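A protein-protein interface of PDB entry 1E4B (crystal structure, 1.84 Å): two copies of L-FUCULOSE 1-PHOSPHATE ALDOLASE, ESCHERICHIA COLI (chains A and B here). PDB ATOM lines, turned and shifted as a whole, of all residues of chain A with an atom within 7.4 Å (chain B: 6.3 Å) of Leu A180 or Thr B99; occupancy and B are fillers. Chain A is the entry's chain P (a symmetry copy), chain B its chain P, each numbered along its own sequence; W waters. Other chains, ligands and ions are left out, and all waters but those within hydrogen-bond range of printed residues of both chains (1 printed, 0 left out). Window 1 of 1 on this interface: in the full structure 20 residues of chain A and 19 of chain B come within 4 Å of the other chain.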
ATOM      1  N   HIS A  97      -2.342   1.836 -31.318  1.00  0.00           N
ATOM      2  CA  HIS A  97      -3.411   2.769 -30.946  1.00  0.00           C
ATOM      3  C   HIS A  97      -2.980   3.695 -29.833  1.00  0.00           C
ATOM      4  O   HIS A  97      -3.226   4.913 -29.889  1.00  0.00           O
ATOM      5  CB  HIS A  97      -4.705   1.991 -30.632  1.00  0.00           C
ATOM      6  CG  HIS A  97      -5.155   1.212 -31.850  1.00  0.00           C
ATOM      7  ND1 HIS A  97      -4.981  -0.142 -31.954  1.00  0.00           N
ATOM      8  CD2 HIS A  97      -5.753   1.606 -32.992  1.00  0.00           C
ATOM      9  CE1 HIS A  97      -5.469  -0.565 -33.109  1.00  0.00           C
ATOM     10  NE2 HIS A  97      -5.940   0.483 -33.775  1.00  0.00           N
ATOM     11  N   ILE A 108      -6.558   9.987 -22.568  1.00  0.00           N
ATOM     12  CA  ILE A 108      -7.765   9.250 -22.956  1.00  0.00           C
ATOM     13  C   ILE A 108      -8.781   9.524 -21.831  1.00  0.00           C
ATOM     14  O   ILE A 108      -8.438   9.222 -20.695  1.00  0.00           O
ATOM     15  CB  ILE A 108      -7.508   7.739 -22.981  1.00  0.00           C
ATOM     16  CG1 ILE A 108      -6.310   7.438 -23.893  1.00  0.00           C
ATOM     17  CG2 ILE A 108      -8.797   7.019 -23.389  1.00  0.00           C
ATOM     18  CD1 ILE A 108      -6.086   5.970 -24.124  1.00  0.00           C
ATOM     19  N   ILE A 111     -14.330   7.397 -21.667  1.00  0.00           N
ATOM     20  CA  ILE A 111     -15.248   6.940 -22.693  1.00  0.00           C
ATOM     21  C   ILE A 111     -15.829   5.561 -22.398  1.00  0.00           C
ATOM     22  O   ILE A 111     -16.758   5.149 -23.081  1.00  0.00           O
ATOM     23  CB  ILE A 111     -14.539   6.895 -24.072  1.00  0.00           C
ATOM     24  CG1 ILE A 111     -13.378   5.900 -24.082  1.00  0.00           C
ATOM     25  CG2 ILE A 111     -14.045   8.305 -24.401  1.00  0.00           C
ATOM     26  CD1 ILE A 111     -12.752   5.719 -25.459  1.00  0.00           C
ATOM     27  N   HIS A 112     -15.274   4.839 -21.439  1.00  0.00           N
ATOM     28  CA  HIS A 112     -15.651   3.486 -21.076  1.00  0.00           C
ATOM     29  C   HIS A 112     -15.374   3.276 -19.590  1.00  0.00           C
ATOM     30  O   HIS A 112     -14.417   3.902 -19.089  1.00  0.00           O
ATOM     31  CB  HIS A 112     -14.855   2.468 -21.914  1.00  0.00           C
ATOM     32  CG  HIS A 112     -15.419   1.088 -21.851  1.00  0.00           C
ATOM     33  ND1 HIS A 112     -15.157   0.235 -20.805  1.00  0.00           N
ATOM     34  CD2 HIS A 112     -16.234   0.416 -22.723  1.00  0.00           C
ATOM     35  CE1 HIS A 112     -15.811  -0.905 -21.014  1.00  0.00           C
ATOM     36  NE2 HIS A 112     -16.458  -0.819 -22.155  1.00  0.00           N
ATOM     37  N   GLU A 173      -5.583  -3.554 -21.979  1.00  0.00           N
ATOM     38  CA  GLU A 173      -6.813  -2.801 -21.797  1.00  0.00           C
ATOM     39  C   GLU A 173      -6.673  -1.342 -22.250  1.00  0.00           C
ATOM     40  O   GLU A 173      -7.628  -0.747 -22.761  1.00  0.00           O
ATOM     41  CB  GLU A 173      -7.290  -2.882 -20.346  1.00  0.00           C
ATOM     42  CG  GLU A 173      -8.603  -2.157 -20.092  1.00  0.00           C
ATOM     43  CD  GLU A 173      -9.772  -2.778 -20.854  1.00  0.00           C
ATOM     44  OE1 GLU A 173      -9.891  -4.025 -20.784  1.00  0.00           O
ATOM     45  OE2 GLU A 173     -10.474  -1.948 -21.500  1.00  0.00           O
ATOM     46  N   VAL A 174      -5.526  -0.736 -21.987  1.00  0.00           N
ATOM     47  CA  VAL A 174      -5.258   0.621 -22.400  1.00  0.00           C
ATOM     48  C   VAL A 174      -5.175   0.686 -23.923  1.00  0.00           C
ATOM     49  O   VAL A 174      -5.715   1.623 -24.527  1.00  0.00           O
ATOM     50  CB  VAL A 174      -4.000   1.207 -21.736  1.00  0.00           C
ATOM     51  CG1 VAL A 174      -3.772   2.611 -22.278  1.00  0.00           C
ATOM     52  CG2 VAL A 174      -4.135   1.198 -20.217  1.00  0.00           C
ATOM     53  N   GLU A 175      -4.597  -0.339 -24.566  1.00  0.00           N
ATOM     54  CA  GLU A 175      -4.593  -0.316 -26.046  1.00  0.00           C
ATOM     55  C   GLU A 175      -6.024  -0.421 -26.575  1.00  0.00           C
ATOM     56  O   GLU A 175      -6.415   0.194 -27.584  1.00  0.00           O
ATOM     57  CB  GLU A 175      -3.723  -1.462 -26.566  1.00  0.00           C
ATOM     58  CG  GLU A 175      -3.797  -1.726 -28.067  1.00  0.00           C
ATOM     59  CD  GLU A 175      -3.099  -0.622 -28.849  1.00  0.00           C
ATOM     60  OE1 GLU A 175      -2.657   0.413 -28.277  1.00  0.00           O
ATOM     61  OE2 GLU A 175      -2.984  -0.773 -30.088  1.00  0.00           O
ATOM     62  N   VAL A 176      -6.890  -1.196 -25.919  1.00  0.00           N
ATOM     63  CA  VAL A 176      -8.284  -1.248 -26.370  1.00  0.00           C
ATOM     64  C   VAL A 176      -8.976   0.105 -26.190  1.00  0.00           C
ATOM     65  O   VAL A 176      -9.756   0.526 -27.044  1.00  0.00           O
ATOM     66  CB  VAL A 176      -9.071  -2.354 -25.645  1.00  0.00           C
ATOM     67  CG1 VAL A 176     -10.561  -2.271 -25.917  1.00  0.00           C
ATOM     68  CG2 VAL A 176      -8.538  -3.708 -26.115  1.00  0.00           C
ATOM     69  N   LEU A 177      -8.777   0.746 -25.057  1.00  0.00           N
ATOM     70  CA  LEU A 177      -9.359   2.052 -24.772  1.00  0.00           C
ATOM     71  C   LEU A 177      -8.863   3.072 -25.807  1.00  0.00           C
ATOM     72  O   LEU A 177      -9.621   3.886 -26.289  1.00  0.00           O
ATOM     73  CB  LEU A 177      -8.951   2.473 -23.360  1.00  0.00           C
ATOM     74  CG  LEU A 177      -9.683   1.793 -22.200  1.00  0.00           C
ATOM     75  CD1 LEU A 177      -9.005   2.134 -20.887  1.00  0.00           C
ATOM     76  CD2 LEU A 177     -11.152   2.216 -22.206  1.00  0.00           C
ATOM     77  N   ALA A 178      -7.575   3.018 -26.153  1.00  0.00           N
ATOM     78  CA  ALA A 178      -6.994   3.859 -27.191  1.00  0.00           C
ATOM     79  C   ALA A 178      -7.653   3.630 -28.554  1.00  0.00           C
ATOM     80  O   ALA A 178      -8.050   4.567 -29.265  1.00  0.00           O
ATOM     81  CB  ALA A 178      -5.480   3.564 -27.279  1.00  0.00           C
ATOM     82  N   GLN A 179      -7.887   2.364 -28.917  1.00  0.00           N
ATOM     83  CA  GLN A 179      -8.550   2.083 -30.198  1.00  0.00           C
ATOM     84  C   GLN A 179      -9.989   2.563 -30.171  1.00  0.00           C
ATOM     85  O   GLN A 179     -10.497   3.139 -31.134  1.00  0.00           O
ATOM     86  CB  GLN A 179      -8.453   0.614 -30.578  1.00  0.00           C
ATOM     87  CG  GLN A 179      -9.141   0.263 -31.889  1.00  0.00           C
ATOM     88  CD  GLN A 179      -9.008  -1.194 -32.281  1.00  0.00           C
ATOM     89  OE1 GLN A 179      -8.536  -1.987 -31.485  1.00  0.00           O
ATOM     90  NE2 GLN A 179      -9.438  -1.537 -33.499  1.00  0.00           N
ATOM     91  N   LEU A 180     -10.716   2.388 -29.068  1.00  0.00           N
ATOM     92  CA  LEU A 180     -12.082   2.923 -28.957  1.00  0.00           C
ATOM     93  C   LEU A 180     -12.108   4.445 -29.132  1.00  0.00           C
ATOM     94  O   LEU A 180     -12.938   5.037 -29.826  1.00  0.00           O
ATOM     95  CB  LEU A 180     -12.641   2.587 -27.555  1.00  0.00           C
ATOM     96  CG  LEU A 180     -12.998   1.108 -27.352  1.00  0.00           C
ATOM     97  CD1 LEU A 180     -13.299   0.861 -25.882  1.00  0.00           C
ATOM     98  CD2 LEU A 180     -14.182   0.676 -28.221  1.00  0.00           C
ATOM     99  N   TYR A 181     -11.162   5.134 -28.504  1.00  0.00           N
ATOM    100  CA  TYR A 181     -11.068   6.584 -28.580  1.00  0.00           C
ATOM    101  C   TYR A 181     -10.784   7.076 -29.995  1.00  0.00           C
ATOM    102  O   TYR A 181     -11.455   7.998 -30.469  1.00  0.00           O
ATOM    103  CB  TYR A 181      -9.978   7.081 -27.613  1.00  0.00           C
ATOM    104  CG  TYR A 181      -9.999   8.579 -27.403  1.00  0.00           C
ATOM    105  CD1 TYR A 181     -11.200   9.274 -27.343  1.00  0.00           C
ATOM    106  CD2 TYR A 181      -8.815   9.294 -27.256  1.00  0.00           C
ATOM    107  CE1 TYR A 181     -11.228  10.640 -27.144  1.00  0.00           C
ATOM    108  CE2 TYR A 181      -8.835  10.665 -27.048  1.00  0.00           C
ATOM    109  CZ  TYR A 181     -10.046  11.327 -26.992  1.00  0.00           C
ATOM    110  OH  TYR A 181     -10.086  12.692 -26.794  1.00  0.00           O
ATOM    111  N   LEU A 182      -9.837   6.477 -30.706  1.00  0.00           N
ATOM    112  CA  LEU A 182      -9.525   6.941 -32.054  1.00  0.00           C
ATOM    113  C   LEU A 182     -10.663   6.624 -33.035  1.00  0.00           C
ATOM    114  O   LEU A 182     -10.889   7.370 -33.986  1.00  0.00           O
ATOM    115  CB  LEU A 182      -8.246   6.285 -32.551  1.00  0.00           C
ATOM    116  CG  LEU A 182      -6.931   6.651 -31.875  1.00  0.00           C
ATOM    117  CD1 LEU A 182      -5.946   5.495 -32.105  1.00  0.00           C
ATOM    118  CD2 LEU A 182      -6.385   7.961 -32.395  1.00  0.00           C
ATOM    119  N   THR A 183     -11.306   5.476 -32.831  1.00  0.00           N
ATOM    120  CA  THR A 183     -12.377   5.052 -33.744  1.00  0.00           C
ATOM    121  C   THR A 183     -13.565   6.010 -33.612  1.00  0.00           C
ATOM    122  O   THR A 183     -14.089   6.463 -34.636  1.00  0.00           O
ATOM    123  CB  THR A 183     -12.811   3.607 -33.454  1.00  0.00           C
ATOM    124  OG1 THR A 183     -11.672   2.739 -33.642  1.00  0.00           O
ATOM    125  CG2 THR A 183     -13.905   3.136 -34.394  1.00  0.00           C
ATOM    126  N   THR A 184     -13.885   6.405 -32.386  1.00  0.00           N
ATOM    127  CA  THR A 184     -14.984   7.319 -32.132  1.00  0.00           C
ATOM    128  C   THR A 184     -14.620   8.778 -32.428  1.00  0.00           C
ATOM    129  O   THR A 184     -15.472   9.516 -32.941  1.00  0.00           O
ATOM    130  CB  THR A 184     -15.542   7.180 -30.709  1.00  0.00           C
ATOM    131  OG1 THR A 184     -14.550   7.325 -29.688  1.00  0.00           O
ATOM    132  CG2 THR A 184     -16.160   5.786 -30.522  1.00  0.00           C
ATOM    133  N   LEU A 185     -13.369   9.173 -32.199  1.00  0.00           N
ATOM    134  CA  LEU A 185     -12.920  10.530 -32.485  1.00  0.00           C
ATOM    135  C   LEU A 185     -12.984  10.869 -33.970  1.00  0.00           C
ATOM    136  O   LEU A 185     -13.199  12.017 -34.353  1.00  0.00           O
ATOM    137  CB  LEU A 185     -11.473  10.713 -32.018  1.00  0.00           C
ATOM    138  CG  LEU A 185     -10.942  12.037 -31.507  1.00  0.00           C
ATOM    139  CD1 LEU A 185     -11.864  12.742 -30.538  1.00  0.00           C
ATOM    140  CD2 LEU A 185      -9.561  11.816 -30.854  1.00  0.00           C
ATOM    141  N   ALA A 186     -12.795   9.881 -34.842  1.00  0.00           N
ATOM    142  CA  ALA A 186     -12.883  10.078 -36.285  1.00  0.00           C
ATOM    143  C   ALA A 186     -14.289  10.449 -36.739  1.00  0.00           C
ATOM    144  O   ALA A 186     -14.489  11.066 -37.785  1.00  0.00           O
ATOM    145  CB  ALA A 186     -12.420   8.807 -36.997  1.00  0.00           C
ATOM    146  N   VAL A 191     -15.776  13.177 -27.954  1.00  0.00           N
ATOM    147  CA  VAL A 191     -16.445  11.898 -27.765  1.00  0.00           C
ATOM    148  C   VAL A 191     -17.212  11.931 -26.440  1.00  0.00           C
ATOM    149  O   VAL A 191     -16.650  12.392 -25.463  1.00  0.00           O
ATOM    150  CB  VAL A 191     -15.431  10.735 -27.668  1.00  0.00           C
ATOM    151  CG1 VAL A 191     -16.198   9.420 -27.495  1.00  0.00           C
ATOM    152  CG2 VAL A 191     -14.558  10.672 -28.914  1.00  0.00           C
ATOM    153  N   ASN B  93     -19.620  -9.572 -24.230  1.00  0.00           N
ATOM    154  CA  ASN B  93     -18.216  -9.246 -24.405  1.00  0.00           C
ATOM    155  C   ASN B  93     -18.137  -7.734 -24.588  1.00  0.00           C
ATOM    156  O   ASN B  93     -19.159  -7.047 -24.640  1.00  0.00           O
ATOM    157  CB  ASN B  93     -17.566  -9.936 -25.588  1.00  0.00           C
ATOM    158  CG  ASN B  93     -18.247  -9.651 -26.913  1.00  0.00           C
ATOM    159  OD1 ASN B  93     -18.581  -8.518 -27.239  1.00  0.00           O
ATOM    160  ND2 ASN B  93     -18.468 -10.719 -27.684  1.00  0.00           N
ATOM    161  N   HIS B  94     -16.905  -7.279 -24.627  1.00  0.00           N
ATOM    162  CA  HIS B  94     -16.649  -5.863 -24.847  1.00  0.00           C
ATOM    163  C   HIS B  94     -15.894  -5.740 -26.174  1.00  0.00           C
ATOM    164  O   HIS B  94     -14.914  -5.008 -26.230  1.00  0.00           O
ATOM    165  CB  HIS B  94     -15.880  -5.230 -23.701  1.00  0.00           C
ATOM    166  CG  HIS B  94     -16.439  -5.318 -22.314  1.00  0.00           C
ATOM    167  ND1 HIS B  94     -15.768  -4.758 -21.240  1.00  0.00           N
ATOM    168  CD2 HIS B  94     -17.586  -5.822 -21.802  1.00  0.00           C
ATOM    169  CE1 HIS B  94     -16.466  -4.990 -20.122  1.00  0.00           C
ATOM    170  NE2 HIS B  94     -17.588  -5.634 -20.462  1.00  0.00           N
ATOM    171  N   ALA B  95     -16.377  -6.348 -27.238  1.00  0.00           N
ATOM    172  CA  ALA B  95     -15.771  -6.343 -28.569  1.00  0.00           C
ATOM    173  C   ALA B  95     -15.617  -4.895 -29.043  1.00  0.00           C
ATOM    174  O   ALA B  95     -16.509  -4.047 -28.836  1.00  0.00           O
ATOM    175  CB  ALA B  95     -16.682  -7.153 -29.496  1.00  0.00           C
ATOM    176  N   VAL B  96     -14.483  -4.578 -29.653  1.00  0.00           N
ATOM    177  CA  VAL B  96     -14.136  -3.181 -29.874  1.00  0.00           C
ATOM    178  C   VAL B  96     -15.119  -2.446 -30.758  1.00  0.00           C
ATOM    179  O   VAL B  96     -15.494  -1.329 -30.365  1.00  0.00           O
ATOM    180  CB  VAL B  96     -12.662  -3.086 -30.331  1.00  0.00           C
ATOM    181  CG1 VAL B  96     -12.338  -4.085 -31.429  1.00  0.00           C
ATOM    182  CG2 VAL B  96     -12.297  -1.675 -30.777  1.00  0.00           C
ATOM    183  N   HIS B  97     -15.542  -3.009 -31.895  1.00  0.00           N
ATOM    184  CA  HIS B  97     -16.434  -2.247 -32.777  1.00  0.00           C
ATOM    185  C   HIS B  97     -17.800  -2.059 -32.160  1.00  0.00           C
ATOM    186  O   HIS B  97     -18.366  -0.952 -32.195  1.00  0.00           O
ATOM    187  CB  HIS B  97     -16.475  -2.897 -34.175  1.00  0.00           C
ATOM    188  CG  HIS B  97     -15.091  -2.904 -34.788  1.00  0.00           C
ATOM    189  ND1 HIS B  97     -14.328  -4.040 -34.852  1.00  0.00           N
ATOM    190  CD2 HIS B  97     -14.354  -1.921 -35.345  1.00  0.00           C
ATOM    191  CE1 HIS B  97     -13.174  -3.767 -35.440  1.00  0.00           C
ATOM    192  NE2 HIS B  97     -13.153  -2.474 -35.744  1.00  0.00           N
ATOM    193  N   CYS B  98     -18.366  -3.123 -31.581  1.00  0.00           N
ATOM    194  CA  CYS B  98     -19.635  -2.998 -30.862  1.00  0.00           C
ATOM    195  C   CYS B  98     -19.556  -1.926 -29.769  1.00  0.00           C
ATOM    196  O   CYS B  98     -20.440  -1.094 -29.616  1.00  0.00           O
ATOM    197  CB  CYS B  98     -19.962  -4.303 -30.138  1.00  0.00           C
ATOM    198  SG  CYS B  98     -20.599  -5.569 -31.259  1.00  0.00           S
ATOM    199  N   THR B  99     -18.488  -2.002 -28.976  1.00  0.00           N
ATOM    200  CA  THR B  99     -18.295  -1.034 -27.882  1.00  0.00           C
ATOM    201  C   THR B  99     -18.133   0.371 -28.410  1.00  0.00           C
ATOM    202  O   THR B  99     -18.683   1.318 -27.808  1.00  0.00           O
ATOM    203  CB  THR B  99     -17.107  -1.530 -27.029  1.00  0.00           C
ATOM    204  OG1 THR B  99     -17.411  -2.878 -26.609  1.00  0.00           O
ATOM    205  CG2 THR B  99     -16.898  -0.637 -25.822  1.00  0.00           C
ATOM    206  N   ALA B 100     -17.407   0.571 -29.529  1.00  0.00           N
ATOM    207  CA  ALA B 100     -17.263   1.923 -30.085  1.00  0.00           C
ATOM    208  C   ALA B 100     -18.626   2.478 -30.494  1.00  0.00           C
ATOM    209  O   ALA B 100     -18.940   3.635 -30.204  1.00  0.00           O
ATOM    210  CB  ALA B 100     -16.272   1.958 -31.256  1.00  0.00           C
ATOM    211  N   VAL B 101     -19.490   1.653 -31.114  1.00  0.00           N
ATOM    212  CA  VAL B 101     -20.836   2.121 -31.441  1.00  0.00           C
ATOM    213  C   VAL B 101     -21.606   2.411 -30.161  1.00  0.00           C
ATOM    214  O   VAL B 101     -22.263   3.461 -30.132  1.00  0.00           O
ATOM    215  CB  VAL B 101     -21.629   1.142 -32.314  1.00  0.00           C
ATOM    216  CG1 VAL B 101     -23.017   1.697 -32.664  1.00  0.00           C
ATOM    217  CG2 VAL B 101     -20.831   0.895 -33.589  1.00  0.00           C
ATOM    218  N   SER B 102     -21.412   1.621 -29.105  1.00  0.00           N
ATOM    219  CA  SER B 102     -22.127   1.893 -27.843  1.00  0.00           C
ATOM    220  C   SER B 102     -21.688   3.199 -27.197  1.00  0.00           C
ATOM    221  O   SER B 102     -22.464   3.825 -26.459  1.00  0.00           O
ATOM    222  CB  SER B 102     -21.878   0.733 -26.876  1.00  0.00           C
ATOM    223  OG  SER B 102     -20.746   0.999 -26.068  1.00  0.00           O
ATOM    224  N   ILE B 103     -20.444   3.619 -27.443  1.00  0.00           N
ATOM    225  CA  ILE B 103     -19.966   4.906 -26.920  1.00  0.00           C
ATOM    226  C   ILE B 103     -20.660   6.079 -27.588  1.00  0.00           C
ATOM    227  O   ILE B 103     -21.003   7.103 -26.980  1.00  0.00           O
ATOM    228  CB  ILE B 103     -18.435   4.987 -27.068  1.00  0.00           C
ATOM    229  CG1 ILE B 103     -17.817   4.039 -26.031  1.00  0.00           C
ATOM    230  CG2 ILE B 103     -17.889   6.397 -26.859  1.00  0.00           C
ATOM    231  CD1 ILE B 103     -16.351   3.738 -26.287  1.00  0.00           C
ATOM    232  N   LEU B 104     -20.995   5.969 -28.864  1.00  0.00           N
ATOM    233  CA  LEU B 104     -21.712   6.979 -29.623  1.00  0.00           C
ATOM    234  C   LEU B 104     -23.193   6.961 -29.263  1.00  0.00           C
ATOM    235  O   LEU B 104     -23.940   7.836 -29.677  1.00  0.00           O
ATOM    236  CB  LEU B 104     -21.527   6.764 -31.141  1.00  0.00           C
ATOM    237  CG  LEU B 104     -20.063   6.792 -31.607  1.00  0.00           C
ATOM    238  CD1 LEU B 104     -19.904   6.411 -33.073  1.00  0.00           C
ATOM    239  CD2 LEU B 104     -19.444   8.162 -31.351  1.00  0.00           C
ATOM    240  N   LEU B 151     -26.639  -3.559 -27.905  1.00  0.00           N
ATOM    241  CA  LEU B 151     -25.409  -2.916 -27.417  1.00  0.00           C
ATOM    242  C   LEU B 151     -25.739  -2.361 -26.035  1.00  0.00           C
ATOM    243  O   LEU B 151     -26.909  -2.286 -25.648  1.00  0.00           O
ATOM    244  CB  LEU B 151     -24.960  -1.772 -28.340  1.00  0.00           C
ATOM    245  CG  LEU B 151     -24.774  -2.238 -29.801  1.00  0.00           C
ATOM    246  CD1 LEU B 151     -24.407  -1.048 -30.665  1.00  0.00           C
ATOM    247  CD2 LEU B 151     -23.710  -3.332 -29.886  1.00  0.00           C
ATOM    248  N   LEU B 152     -24.705  -2.088 -25.240  1.00  0.00           N
ATOM    249  CA  LEU B 152     -24.889  -1.516 -23.904  1.00  0.00           C
ATOM    250  C   LEU B 152     -24.054  -0.225 -23.934  1.00  0.00           C
ATOM    251  O   LEU B 152     -22.850  -0.337 -24.149  1.00  0.00           O
ATOM    252  CB  LEU B 152     -24.327  -2.466 -22.851  1.00  0.00           C
ATOM    253  CG  LEU B 152     -25.132  -3.714 -22.473  1.00  0.00           C
ATOM    254  CD1 LEU B 152     -25.128  -4.725 -23.598  1.00  0.00           C
ATOM    255  CD2 LEU B 152     -24.513  -4.376 -21.244  1.00  0.00           C
ATOM    256  N   HIS B 154     -21.576   2.753 -23.536  1.00  0.00           N
ATOM    257  CA  HIS B 154     -20.310   2.836 -22.826  1.00  0.00           C
ATOM    258  C   HIS B 154     -19.851   1.512 -22.220  1.00  0.00           C
ATOM    259  O   HIS B 154     -19.187   1.490 -21.167  1.00  0.00           O
ATOM    260  CB  HIS B 154     -20.337   3.884 -21.696  1.00  0.00           C
ATOM    261  CG  HIS B 154     -20.411   5.292 -22.175  1.00  0.00           C
ATOM    262  ND1 HIS B 154     -19.363   5.956 -22.786  1.00  0.00           N
ATOM    263  CD2 HIS B 154     -21.425   6.192 -22.086  1.00  0.00           C
ATOM    264  CE1 HIS B 154     -19.759   7.192 -23.080  1.00  0.00           C
ATOM    265  NE2 HIS B 154     -21.001   7.366 -22.655  1.00  0.00           N
ATOM    266  N   HIS B 155     -20.157   0.384 -22.913  1.00  0.00           N
ATOM    267  CA  HIS B 155     -19.890  -0.893 -22.257  1.00  0.00           C
ATOM    268  C   HIS B 155     -19.612  -2.029 -23.224  1.00  0.00           C
ATOM    269  O   HIS B 155     -18.477  -2.507 -23.170  1.00  0.00           O
ATOM    270  CB  HIS B 155     -21.087  -1.227 -21.349  1.00  0.00           C
ATOM    271  CG  HIS B 155     -20.915  -2.437 -20.491  1.00  0.00           C
ATOM    272  ND1 HIS B 155     -21.487  -2.531 -19.237  1.00  0.00           N
ATOM    273  CD2 HIS B 155     -20.218  -3.596 -20.654  1.00  0.00           C
ATOM    274  CE1 HIS B 155     -21.140  -3.677 -18.701  1.00  0.00           C
ATOM    275  NE2 HIS B 155     -20.401  -4.378 -19.541  1.00  0.00           N
ATOM    276  N   GLY B 156     -20.582  -2.490 -24.010  1.00  0.00           N
ATOM    277  CA  GLY B 156     -20.271  -3.664 -24.850  1.00  0.00           C
ATOM    278  C   GLY B 156     -21.527  -4.257 -25.480  1.00  0.00           C
ATOM    279  O   GLY B 156     -22.426  -3.515 -25.877  1.00  0.00           O
ATOM    280  N   LEU B 157     -21.571  -5.580 -25.544  1.00  0.00           N
ATOM    281  CA  LEU B 157     -22.639  -6.280 -26.257  1.00  0.00           C
ATOM    282  C   LEU B 157     -23.160  -7.463 -25.468  1.00  0.00           C
ATOM    283  O   LEU B 157     -22.383  -8.144 -24.792  1.00  0.00           O
ATOM    284  CB  LEU B 157     -21.936  -6.817 -27.533  1.00  0.00           C
ATOM    285  CG  LEU B 157     -22.577  -7.714 -28.584  1.00  0.00           C
ATOM    286  CD1 LEU B 157     -22.754  -9.138 -28.103  1.00  0.00           C
ATOM    287  CD2 LEU B 157     -23.912  -7.231 -29.115  1.00  0.00           C
ATOM    288  N   GLU B 175     -20.611  -7.909 -34.285  1.00  0.00           N
ATOM    289  CA  GLU B 175     -19.336  -7.158 -34.322  1.00  0.00           C
ATOM    290  C   GLU B 175     -18.984  -6.795 -35.765  1.00  0.00           C
ATOM    291  O   GLU B 175     -18.447  -5.716 -36.075  1.00  0.00           O
ATOM    292  CB  GLU B 175     -18.235  -8.003 -33.678  1.00  0.00           C
ATOM    293  CG  GLU B 175     -16.811  -7.479 -33.841  1.00  0.00           C
ATOM    294  CD  GLU B 175     -16.587  -6.238 -32.987  1.00  0.00           C
ATOM    295  OE1 GLU B 175     -17.534  -5.691 -32.358  1.00  0.00           O
ATOM    296  OE2 GLU B 175     -15.425  -5.771 -32.938  1.00  0.00           O
ATOM    297  N   ALA B 178     -21.180  -3.840 -36.689  1.00  0.00           N
ATOM    298  CA  ALA B 178     -20.619  -2.683 -36.004  1.00  0.00           C
ATOM    299  C   ALA B 178     -19.397  -2.118 -36.734  1.00  0.00           C
ATOM    300  O   ALA B 178     -19.275  -0.909 -36.985  1.00  0.00           O
ATOM    301  CB  ALA B 178     -20.233  -3.096 -34.567  1.00  0.00           C
HETATM  302  O   HOH W   1     -13.085  -3.870 -21.644  1.00  0.00           O
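NE2 of His A112 lies within hydrogen-bond range of O of His B155.
A ring nitrogen (ND1) of His B154 lies within hydrogen-bond range of the backbone carbonyl oxygen (O) of Ile A111 (2.7 Å).
The side-chain hydroxyl (OG1) of Thr A183 lies within hydrogen-bond range of the backbone carbonyl oxygen (O) of Gln A179 (2.8 Å).
O of Thr B99 is in hydrogen-bond range of OG of Ser B102, 2.7 Å away.
O of Leu A180 sits at hydrogen-bond distance from OG1 of Thr A184 (2.8 Å).
O of His B94 lies close to OG1 of Thr B99, 3.3 Å away.
The backbone NH (N) of His B154 sits at hydrogen-bond distance from the side-chain hydroxyl (OG) of Ser B102 (3.2 Å).
The side-chain hydroxyl of Thr A184 is in hydrogen-bond range of the backbone carbonyl oxygen of Tyr A181.
Among the printed residues, merely in contact across the chains: Ile A111 with Ile B103 (3.3 Å), His A112 with His B94 (3.9 Å), His A112 with Thr B99 (3.3 Å), His A112 with His B154 (3.5 Å), Gln A179 with Val B96 (3.6 Å), Leu A180 with Val B96 (3.2 Å), Leu A180 with Thr B99 (3.9 Å), Leu A180 with Ala B100 (3.5 Å), Thr A184 with Ala B100 (3.5 Å) and Val A191 with Ile B103 (3.5 Å).
Printed residues of chain B within 4 Å of Leu A180: Val B96 (3.2 Å), Thr B99 (3.9 Å) and Ala B100 (3.5 Å).
Of the printed residues of chain A, Thr B99 touches His A112 (3.3 Å) and Leu A180 (3.9 Å).
Of the printed residues of chain A, His B154 touches Ile A111 and His A112.
Of the printed residues of chain A, Ile B103 touches Ile A111 and Val A191.
Of the printed residues of chain B, Val A191 touches Ile B103 (3.5 Å).
Of the printed residues of chain A, His B94 touches His A112.
Ala A178 touches none of the printed residues of chain B.
The nearest residue of chain A that does not touch Thr B99 is Thr A184 (5.8 Å).
The nearest printed residue of chain B that does not touch Thr A184 is Leu B104 (4.1 Å).
Of the 20 printed residues of chain B, 7 touch a printed residue of chain A.
Printed residues of chain B that touch a printed residue of chain A: His B94, Val B96, Thr B99, Ala B100, Ile B103, His B154 and His B155.
Among the printed residues, 12 pairs touch across the chains.
3 positions are printed for both chains.
Water W1 lies within hydrogen-bond range of ND1 of His B94 (2.9 Å) and OE2 of Glu A173 (3.2 Å).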
